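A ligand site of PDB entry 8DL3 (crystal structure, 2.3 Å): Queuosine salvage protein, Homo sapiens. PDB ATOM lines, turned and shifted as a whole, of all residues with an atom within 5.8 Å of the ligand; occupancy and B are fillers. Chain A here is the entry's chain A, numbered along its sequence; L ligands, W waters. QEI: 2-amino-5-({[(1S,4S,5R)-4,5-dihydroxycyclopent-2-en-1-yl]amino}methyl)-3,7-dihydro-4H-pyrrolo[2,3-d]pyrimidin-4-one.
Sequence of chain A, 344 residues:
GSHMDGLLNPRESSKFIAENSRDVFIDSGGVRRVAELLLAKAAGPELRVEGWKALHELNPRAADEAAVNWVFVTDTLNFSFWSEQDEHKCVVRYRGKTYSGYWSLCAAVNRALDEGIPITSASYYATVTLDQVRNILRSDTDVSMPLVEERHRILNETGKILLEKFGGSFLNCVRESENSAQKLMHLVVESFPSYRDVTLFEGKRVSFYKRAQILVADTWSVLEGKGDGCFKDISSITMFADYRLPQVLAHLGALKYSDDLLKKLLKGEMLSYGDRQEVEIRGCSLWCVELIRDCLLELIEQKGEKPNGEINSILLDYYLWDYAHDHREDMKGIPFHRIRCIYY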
ATOM      1  N   TRP A  52      -8.156  -8.181 -14.608  1.00  0.00           N
ATOM      2  CA  TRP A  52      -7.018  -8.737 -15.327  1.00  0.00           C
ATOM      3  C   TRP A  52      -5.767  -7.882 -15.058  1.00  0.00           C
ATOM      4  O   TRP A  52      -4.686  -8.411 -14.830  1.00  0.00           O
ATOM      5  CB  TRP A  52      -7.341  -8.854 -16.817  1.00  0.00           C
ATOM      6  CG  TRP A  52      -6.295  -9.544 -17.631  1.00  0.00           C
ATOM      7  CD1 TRP A  52      -6.229 -10.880 -17.923  1.00  0.00           C
ATOM      8  CD2 TRP A  52      -5.173  -8.934 -18.292  1.00  0.00           C
ATOM      9  NE1 TRP A  52      -5.149 -11.139 -18.732  1.00  0.00           N
ATOM     10  CE2 TRP A  52      -4.481  -9.965 -18.968  1.00  0.00           C
ATOM     11  CE3 TRP A  52      -4.701  -7.624 -18.395  1.00  0.00           C
ATOM     12  CZ2 TRP A  52      -3.331  -9.721 -19.723  1.00  0.00           C
ATOM     13  CZ3 TRP A  52      -3.571  -7.386 -19.141  1.00  0.00           C
ATOM     14  CH2 TRP A  52      -2.890  -8.425 -19.791  1.00  0.00           C
ATOM     15  N   HIS A  56      -3.391  -8.449 -11.034  1.00  0.00           N
ATOM     16  CA  HIS A  56      -2.165  -9.097 -11.516  1.00  0.00           C
ATOM     17  C   HIS A  56      -1.125  -8.034 -11.879  1.00  0.00           C
ATOM     18  O   HIS A  56      -1.159  -7.512 -12.979  1.00  0.00           O
ATOM     19  CB  HIS A  56      -2.458 -10.004 -12.709  1.00  0.00           C
ATOM     20  CG  HIS A  56      -3.608 -10.931 -12.488  1.00  0.00           C
ATOM     21  ND1 HIS A  56      -4.844 -10.735 -13.076  1.00  0.00           N
ATOM     22  CD2 HIS A  56      -3.708 -12.033 -11.711  1.00  0.00           C
ATOM     23  CE1 HIS A  56      -5.656 -11.695 -12.675  1.00  0.00           C
ATOM     24  NE2 HIS A  56      -4.981 -12.513 -11.843  1.00  0.00           N
ATOM     25  N   ASN A  59       0.891  -7.964 -15.170  1.00  0.00           N
ATOM     26  CA  ASN A  59       0.208  -7.665 -16.446  1.00  0.00           C
ATOM     27  C   ASN A  59       0.505  -6.216 -16.826  1.00  0.00           C
ATOM     28  O   ASN A  59       0.777  -5.394 -15.958  1.00  0.00           O
ATOM     29  CB  ASN A  59      -1.294  -8.008 -16.417  1.00  0.00           C
ATOM     30  CG  ASN A  59      -1.577  -9.505 -16.518  1.00  0.00           C
ATOM     31  OD1 ASN A  59      -2.686  -9.970 -16.235  1.00  0.00           O
ATOM     32  ND2 ASN A  59      -0.580 -10.265 -16.938  1.00  0.00           N
ATOM     33  N   ASN A  78       2.338 -19.737 -23.730  1.00  0.00           N
ATOM     34  CA  ASN A  78       1.494 -20.015 -22.568  1.00  0.00           C
ATOM     35  C   ASN A  78       1.131 -21.512 -22.575  1.00  0.00           C
ATOM     36  O   ASN A  78       0.017 -21.899 -22.894  1.00  0.00           O
ATOM     37  CB  ASN A  78       0.310 -19.049 -22.523  1.00  0.00           C
ATOM     38  CG  ASN A  78      -0.550 -19.190 -21.281  1.00  0.00           C
ATOM     39  OD1 ASN A  78      -0.402 -20.137 -20.513  1.00  0.00           O
ATOM     40  ND2 ASN A  78      -1.456 -18.250 -21.082  1.00  0.00           N
ATOM     41  N   PHE A  81       3.986 -25.358 -17.628  1.00  0.00           N
ATOM     42  CA  PHE A  81       4.852 -24.762 -16.616  1.00  0.00           C
ATOM     43  C   PHE A  81       5.010 -25.683 -15.392  1.00  0.00           C
ATOM     44  O   PHE A  81       5.854 -25.427 -14.547  1.00  0.00           O
ATOM     45  CB  PHE A  81       4.298 -23.386 -16.229  1.00  0.00           C
ATOM     46  CG  PHE A  81       4.220 -22.415 -17.373  1.00  0.00           C
ATOM     47  CD1 PHE A  81       5.352 -21.778 -17.857  1.00  0.00           C
ATOM     48  CD2 PHE A  81       2.997 -22.154 -17.992  1.00  0.00           C
ATOM     49  CE1 PHE A  81       5.280 -20.907 -18.928  1.00  0.00           C
ATOM     50  CE2 PHE A  81       2.931 -21.269 -19.053  1.00  0.00           C
ATOM     51  CZ  PHE A  81       4.064 -20.641 -19.516  1.00  0.00           C
ATOM     52  N   TYR A 102       3.334 -20.090 -14.885  1.00  0.00           N
ATOM     53  CA  TYR A 102       3.127 -19.139 -15.970  1.00  0.00           C
ATOM     54  C   TYR A 102       3.600 -17.737 -15.548  1.00  0.00           C
ATOM     55  O   TYR A 102       4.182 -17.021 -16.361  1.00  0.00           O
ATOM     56  CB  TYR A 102       1.665 -19.153 -16.432  1.00  0.00           C
ATOM     57  CG  TYR A 102       1.250 -17.950 -17.228  1.00  0.00           C
ATOM     58  CD1 TYR A 102       1.689 -17.764 -18.531  1.00  0.00           C
ATOM     59  CD2 TYR A 102       0.460 -16.965 -16.667  1.00  0.00           C
ATOM     60  CE1 TYR A 102       1.324 -16.650 -19.263  1.00  0.00           C
ATOM     61  CE2 TYR A 102       0.107 -15.825 -17.378  1.00  0.00           C
ATOM     62  CZ  TYR A 102       0.531 -15.673 -18.690  1.00  0.00           C
ATOM     63  OH  TYR A 102       0.181 -14.568 -19.407  1.00  0.00           O
ATOM     64  N   TRP A 103       3.376 -17.327 -14.294  1.00  0.00           N
ATOM     65  CA  TRP A 103       3.776 -15.976 -13.854  1.00  0.00           C
ATOM     66  C   TRP A 103       5.297 -15.752 -13.942  1.00  0.00           C
ATOM     67  O   TRP A 103       5.722 -14.596 -14.108  1.00  0.00           O
ATOM     68  CB  TRP A 103       3.285 -15.660 -12.440  1.00  0.00           C
ATOM     69  CG  TRP A 103       1.822 -15.380 -12.405  1.00  0.00           C
ATOM     70  CD1 TRP A 103       0.887 -15.995 -11.633  1.00  0.00           C
ATOM     71  CD2 TRP A 103       1.107 -14.445 -13.237  1.00  0.00           C
ATOM     72  NE1 TRP A 103      -0.357 -15.504 -11.900  1.00  0.00           N
ATOM     73  CE2 TRP A 103      -0.256 -14.542 -12.886  1.00  0.00           C
ATOM     74  CE3 TRP A 103       1.480 -13.530 -14.225  1.00  0.00           C
ATOM     75  CZ2 TRP A 103      -1.244 -13.770 -13.485  1.00  0.00           C
ATOM     76  CZ3 TRP A 103       0.508 -12.760 -14.821  1.00  0.00           C
ATOM     77  CH2 TRP A 103      -0.841 -12.881 -14.457  1.00  0.00           C
ATOM     78  N   LYS A 210      -6.773 -23.455 -26.970  1.00  0.00           N
ATOM     79  CA  LYS A 210      -6.531 -22.881 -25.650  1.00  0.00           C
ATOM     80  C   LYS A 210      -5.760 -21.566 -25.818  1.00  0.00           C
ATOM     81  O   LYS A 210      -6.231 -20.498 -25.422  1.00  0.00           O
ATOM     82  CB  LYS A 210      -5.780 -23.875 -24.754  1.00  0.00           C
ATOM     83  CG  LYS A 210      -5.437 -23.352 -23.366  1.00  0.00           C
ATOM     84  CD  LYS A 210      -4.075 -22.716 -23.246  1.00  0.00           C
ATOM     85  CE  LYS A 210      -3.791 -22.151 -21.870  1.00  0.00           C
ATOM     86  NZ  LYS A 210      -2.330 -22.078 -21.612  1.00  0.00           N
ATOM     87  N   ILE A 214      -7.202 -17.789 -25.334  1.00  0.00           N
ATOM     88  CA  ILE A 214      -6.732 -16.970 -24.237  1.00  0.00           C
ATOM     89  C   ILE A 214      -6.058 -15.724 -24.824  1.00  0.00           C
ATOM     90  O   ILE A 214      -6.153 -14.638 -24.238  1.00  0.00           O
ATOM     91  CB  ILE A 214      -5.816 -17.710 -23.242  1.00  0.00           C
ATOM     92  CG1 ILE A 214      -5.720 -16.928 -21.937  1.00  0.00           C
ATOM     93  CG2 ILE A 214      -4.450 -17.972 -23.819  1.00  0.00           C
ATOM     94  CD1 ILE A 214      -5.172 -17.711 -20.771  1.00  0.00           C
ATOM     95  N   ASP A 218      -7.044 -12.095 -23.774  1.00  0.00           N
ATOM     96  CA  ASP A 218      -6.007 -11.276 -23.161  1.00  0.00           C
ATOM     97  C   ASP A 218      -5.827  -9.969 -23.928  1.00  0.00           C
ATOM     98  O   ASP A 218      -5.411  -8.953 -23.338  1.00  0.00           O
ATOM     99  CB  ASP A 218      -4.683 -12.052 -23.070  1.00  0.00           C
ATOM    100  CG  ASP A 218      -4.636 -13.035 -21.923  1.00  0.00           C
ATOM    101  OD1 ASP A 218      -5.547 -13.003 -21.080  1.00  0.00           O
ATOM    102  OD2 ASP A 218      -3.683 -13.829 -21.880  1.00  0.00           O
ATOM    103  N   MET A 239     -13.831 -21.139 -22.259  1.00  0.00           N
ATOM    104  CA  MET A 239     -12.716 -21.288 -21.328  1.00  0.00           C
ATOM    105  C   MET A 239     -11.525 -21.807 -22.122  1.00  0.00           C
ATOM    106  O   MET A 239     -11.678 -22.275 -23.270  1.00  0.00           O
ATOM    107  CB  MET A 239     -13.040 -22.230 -20.154  1.00  0.00           C
ATOM    108  CG  MET A 239     -13.316 -23.658 -20.574  1.00  0.00           C
ATOM    109  SD  MET A 239     -11.845 -24.742 -20.727  1.00  0.00           S
ATOM    110  CE  MET A 239     -11.423 -24.968 -18.993  1.00  0.00           C
ATOM    111  N   PHE A 240     -10.344 -21.708 -21.504  1.00  0.00           N
ATOM    112  CA  PHE A 240      -9.095 -22.073 -22.162  1.00  0.00           C
ATOM    113  C   PHE A 240      -8.659 -23.413 -21.549  1.00  0.00           C
ATOM    114  O   PHE A 240      -8.221 -23.457 -20.403  1.00  0.00           O
ATOM    115  CB  PHE A 240      -8.069 -20.943 -22.029  1.00  0.00           C
ATOM    116  CG  PHE A 240      -8.683 -19.583 -21.894  1.00  0.00           C
ATOM    117  CD1 PHE A 240      -9.403 -19.028 -22.951  1.00  0.00           C
ATOM    118  CD2 PHE A 240      -8.599 -18.877 -20.705  1.00  0.00           C
ATOM    119  CE1 PHE A 240      -9.987 -17.778 -22.823  1.00  0.00           C
ATOM    120  CE2 PHE A 240      -9.195 -17.632 -20.583  1.00  0.00           C
ATOM    121  CZ  PHE A 240      -9.881 -17.080 -21.635  1.00  0.00           C
ATOM    122  N   ALA A 241      -8.841 -24.478 -22.335  1.00  0.00           N
ATOM    123  CA  ALA A 241      -8.798 -25.830 -21.815  1.00  0.00           C
ATOM    124  C   ALA A 241      -7.333 -26.235 -21.543  1.00  0.00           C
ATOM    125  O   ALA A 241      -6.635 -26.664 -22.435  1.00  0.00           O
ATOM    126  CB  ALA A 241      -9.479 -26.768 -22.781  1.00  0.00           C
ATOM    127  N   ASP A 242      -6.914 -26.109 -20.276  1.00  0.00           N
ATOM    128  CA  ASP A 242      -5.515 -26.363 -19.864  1.00  0.00           C
ATOM    129  C   ASP A 242      -5.495 -27.517 -18.849  1.00  0.00           C
ATOM    130  O   ASP A 242      -6.369 -28.393 -18.877  1.00  0.00           O
ATOM    131  CB  ASP A 242      -4.906 -25.058 -19.363  1.00  0.00           C
ATOM    132  CG  ASP A 242      -5.276 -24.742 -17.928  1.00  0.00           C
ATOM    133  OD1 ASP A 242      -6.445 -24.951 -17.572  1.00  0.00           O
ATOM    134  OD2 ASP A 242      -4.363 -24.351 -17.165  1.00  0.00           O
ATOM    135  N   LEU A 245      -7.514 -25.768 -14.886  1.00  0.00           N
ATOM    136  CA  LEU A 245      -8.954 -25.545 -14.780  1.00  0.00           C
ATOM    137  C   LEU A 245      -9.683 -26.852 -14.509  1.00  0.00           C
ATOM    138  O   LEU A 245     -10.591 -26.875 -13.686  1.00  0.00           O
ATOM    139  CB  LEU A 245      -9.480 -24.850 -16.036  1.00  0.00           C
ATOM    140  CG  LEU A 245     -10.016 -23.448 -15.811  1.00  0.00           C
ATOM    141  CD1 LEU A 245     -11.332 -23.484 -15.050  1.00  0.00           C
ATOM    142  CD2 LEU A 245      -8.990 -22.579 -15.097  1.00  0.00           C
ATOM    143  N   ASP A 317     -13.335 -18.420 -16.219  1.00  0.00           N
ATOM    144  CA  ASP A 317     -12.078 -19.095 -16.406  1.00  0.00           C
ATOM    145  C   ASP A 317     -10.978 -18.344 -15.642  1.00  0.00           C
ATOM    146  O   ASP A 317     -10.340 -18.918 -14.783  1.00  0.00           O
ATOM    147  CB  ASP A 317     -11.754 -19.218 -17.895  1.00  0.00           C
ATOM    148  CG  ASP A 317     -10.382 -19.799 -18.148  1.00  0.00           C
ATOM    149  OD1 ASP A 317      -9.409 -19.216 -17.624  1.00  0.00           O
ATOM    150  OD2 ASP A 317     -10.299 -20.826 -18.844  1.00  0.00           O
ATOM    151  N   TYR A 318     -10.780 -17.068 -15.964  1.00  0.00           N
ATOM    152  CA  TYR A 318      -9.761 -16.247 -15.276  1.00  0.00           C
ATOM    153  C   TYR A 318      -9.899 -16.429 -13.760  1.00  0.00           C
ATOM    154  O   TYR A 318      -8.903 -16.618 -13.067  1.00  0.00           O
ATOM    155  CB  TYR A 318      -9.868 -14.738 -15.556  1.00  0.00           C
ATOM    156  CG  TYR A 318      -9.408 -14.215 -16.904  1.00  0.00           C
ATOM    157  CD1 TYR A 318      -8.451 -14.842 -17.679  1.00  0.00           C
ATOM    158  CD2 TYR A 318      -9.915 -13.010 -17.355  1.00  0.00           C
ATOM    159  CE1 TYR A 318      -8.024 -14.306 -18.886  1.00  0.00           C
ATOM    160  CE2 TYR A 318      -9.504 -12.458 -18.564  1.00  0.00           C
ATOM    161  CZ  TYR A 318      -8.555 -13.106 -19.338  1.00  0.00           C
ATOM    162  OH  TYR A 318      -8.177 -12.539 -20.518  1.00  0.00           O
ATOM    163  N   TYR A 319     -11.144 -16.351 -13.253  1.00  0.00           N
ATOM    164  CA  TYR A 319     -11.389 -16.433 -11.806  1.00  0.00           C
ATOM    165  C   TYR A 319     -10.904 -17.784 -11.285  1.00  0.00           C
ATOM    166  O   TYR A 319     -10.134 -17.852 -10.312  1.00  0.00           O
ATOM    167  CB  TYR A 319     -12.850 -16.269 -11.396  1.00  0.00           C
ATOM    168  CG  TYR A 319     -13.046 -16.430  -9.905  1.00  0.00           C
ATOM    169  CD1 TYR A 319     -12.607 -15.461  -9.019  1.00  0.00           C
ATOM    170  CD2 TYR A 319     -13.602 -17.590  -9.362  1.00  0.00           C
ATOM    171  CE1 TYR A 319     -12.747 -15.604  -7.642  1.00  0.00           C
ATOM    172  CE2 TYR A 319     -13.744 -17.746  -7.986  1.00  0.00           C
ATOM    173  CZ  TYR A 319     -13.323 -16.753  -7.122  1.00  0.00           C
ATOM    174  OH  TYR A 319     -13.459 -16.914  -5.782  1.00  0.00           O
ATOM    175  N   TRP A 321      -8.987 -20.018 -12.525  1.00  0.00           N
ATOM    176  CA  TRP A 321      -7.560 -20.235 -12.691  1.00  0.00           C
ATOM    177  C   TRP A 321      -6.804 -19.687 -11.476  1.00  0.00           C
ATOM    178  O   TRP A 321      -5.880 -20.338 -10.976  1.00  0.00           O
ATOM    179  CB  TRP A 321      -7.051 -19.607 -13.982  1.00  0.00           C
ATOM    180  CG  TRP A 321      -5.679 -20.080 -14.344  1.00  0.00           C
ATOM    181  CD1 TRP A 321      -5.356 -21.177 -15.075  1.00  0.00           C
ATOM    182  CD2 TRP A 321      -4.437 -19.484 -13.948  1.00  0.00           C
ATOM    183  NE1 TRP A 321      -4.001 -21.306 -15.173  1.00  0.00           N
ATOM    184  CE2 TRP A 321      -3.410 -20.278 -14.498  1.00  0.00           C
ATOM    185  CE3 TRP A 321      -4.097 -18.367 -13.186  1.00  0.00           C
ATOM    186  CZ2 TRP A 321      -2.056 -19.983 -14.306  1.00  0.00           C
ATOM    187  CZ3 TRP A 321      -2.760 -18.070 -12.997  1.00  0.00           C
ATOM    188  CH2 TRP A 321      -1.758 -18.869 -13.547  1.00  0.00           C
ATOM    189  N   ASP A 322      -7.182 -18.482 -11.050  1.00  0.00           N
ATOM    190  CA  ASP A 322      -6.545 -17.772  -9.936  1.00  0.00           C
ATOM    191  C   ASP A 322      -6.826 -18.535  -8.649  1.00  0.00           C
ATOM    192  O   ASP A 322      -5.933 -18.781  -7.836  1.00  0.00           O
ATOM    193  CB  ASP A 322      -7.033 -16.313  -9.861  1.00  0.00           C
ATOM    194  CG  ASP A 322      -6.274 -15.329 -10.746  1.00  0.00           C
ATOM    195  OD1 ASP A 322      -5.333 -15.776 -11.445  1.00  0.00           O
ATOM    196  OD2 ASP A 322      -6.610 -14.129 -10.732  1.00  0.00           O
HETATM  197  C1  QEI L   1      -3.914 -15.028 -16.039  1.00  0.00           C
HETATM  198  C2  QEI L   1      -4.747 -15.522 -14.865  1.00  0.00           C
HETATM  199  C3  QEI L   1      -4.531 -13.691 -16.330  1.00  0.00           C
HETATM  200  C4  QEI L   1      -6.110 -14.900 -15.114  1.00  0.00           C
HETATM  201  C5  QEI L   1      -5.733 -13.605 -15.798  1.00  0.00           C
HETATM  202  C6  QEI L   1      -2.880 -16.978 -17.120  1.00  0.00           C
HETATM  203  C9  QEI L   1      -4.496 -19.074 -17.641  1.00  0.00           C
HETATM  204  C10 QEI L   1      -4.165 -20.409 -18.183  1.00  0.00           C
HETATM  205  C11 QEI L   1      -5.901 -18.765 -17.329  1.00  0.00           C
HETATM  206  O1  QEI L   1      -4.190 -15.043 -13.630  1.00  0.00           O
HETATM  207  O2  QEI L   1      -6.902 -14.749 -13.944  1.00  0.00           O
HETATM  208  N1  QEI L   1      -3.988 -16.042 -17.060  1.00  0.00           N
HETATM  209  C7  QEI L   1      -3.194 -18.384 -17.586  1.00  0.00           C
HETATM  210  C8  QEI L   1      -2.254 -19.293 -18.042  1.00  0.00           C
HETATM  211  N2  QEI L   1      -2.839 -20.470 -18.381  1.00  0.00           N
HETATM  212  N3  QEI L   1      -5.183 -21.288 -18.344  1.00  0.00           N
HETATM  213  C12 QEI L   1      -6.477 -20.933 -18.035  1.00  0.00           C
HETATM  214  N5  QEI L   1      -7.455 -21.864 -18.221  1.00  0.00           N
HETATM  215  N4  QEI L   1      -6.804 -19.715 -17.554  1.00  0.00           N
HETATM  216  O3  QEI L   1      -6.238 -17.643 -16.889  1.00  0.00           O
HETATM  217  O   HOH W   1      -3.166 -15.250 -19.508  1.00  0.00           O
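N5 of the ligand lies within hydrogen-bond range of OD1 of Asp 242 (3.3 Å). O of Phe 240 lies within hydrogen-bond range of N5 of the ligand. NE1 of Trp 321 sits close to N3 of the ligand (3.4 Å). An oxygen (O2) of the ligand lies within hydrogen-bond range of the backbone carbonyl oxygen of Tyr 318, 2.9 Å away. The side-chain carboxylate (OD1) of Asp 317 sits at hydrogen-bond distance from a nitrogen (N4) of the ligand, 2.7 Å away. The side-chain amide oxygen (OD1) of Asn 78 sits close to a nitrogen (N2) of the ligand (3.3 Å). OD1 of Asp 322 sits at hydrogen-bond distance from O1 of the ligand, at 2.6 Å. A ring nitrogen (NE2) of His 56 sits at hydrogen-bond distance from an oxygen (O1) of the ligand, at 3.2 Å.
The backbone carbonyl oxygen of Trp 52 lies close to the side-chain amide oxygen of Asn 59 (2.9 Å). A ring nitrogen (NE2) of His 56 is in hydrogen-bond range of the side-chain carboxylate (OD2) of Asp 322, at 2.5 Å. The side-chain amino group (NZ) of Lys 210 lies within hydrogen-bond range of the backbone carbonyl oxygen (O) of Asn 78, at 2.7 Å. OD1 of Asp 218 is in hydrogen-bond range of NE1 of Trp 52, 3.0 Å away. OH of Tyr 318 is in hydrogen-bond range of OD1 of Asp 218 (2.7 Å). OD2 of Asp 317 sits at hydrogen-bond distance from N of Phe 240 (2.8 Å). The side-chain carboxylate (OD1) of Asp 242 lies within hydrogen-bond range of the backbone NH (N) of Leu 245 (3.0 Å). A ring nitrogen (ND1) of His 56 is in hydrogen-bond range of the backbone carbonyl oxygen (O) of Trp 52.
Merely in contact with the ligand: Tyr 102 (3.2 Å), Trp 103 (3.2 Å), Ile 214 (3.5 Å), Trp 52 (3.5 Å), Leu 245 (3.6 Å) and Lys 210 (3.6 Å). Hydrophobic or aromatic side chains that line the ligand: Trp 52, His 56, Tyr 102, Trp 103, Ile 214, Phe 240, Leu 245, Tyr 318 and Trp 321. Within 4 Å of the ligand: Trp 52, His 56, Asn 78, Tyr 102, Trp 103, Lys 210, Ile 214, Phe 240, Asp 242, Leu 245, Asp 317, Tyr 318, Trp 321 and Asp 322. Along chain A the residues within 4 Å of the ligand span positions 52 to 322. The nearest printed residue that does not touch the ligand is Asn 59 (4.2 Å).
Water W1 lies within hydrogen-bond range of N1 of the ligand (2.7 Å), OD2 of Asp 218 (2.8 Å) and OH of Tyr 102 (3.4 Å).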
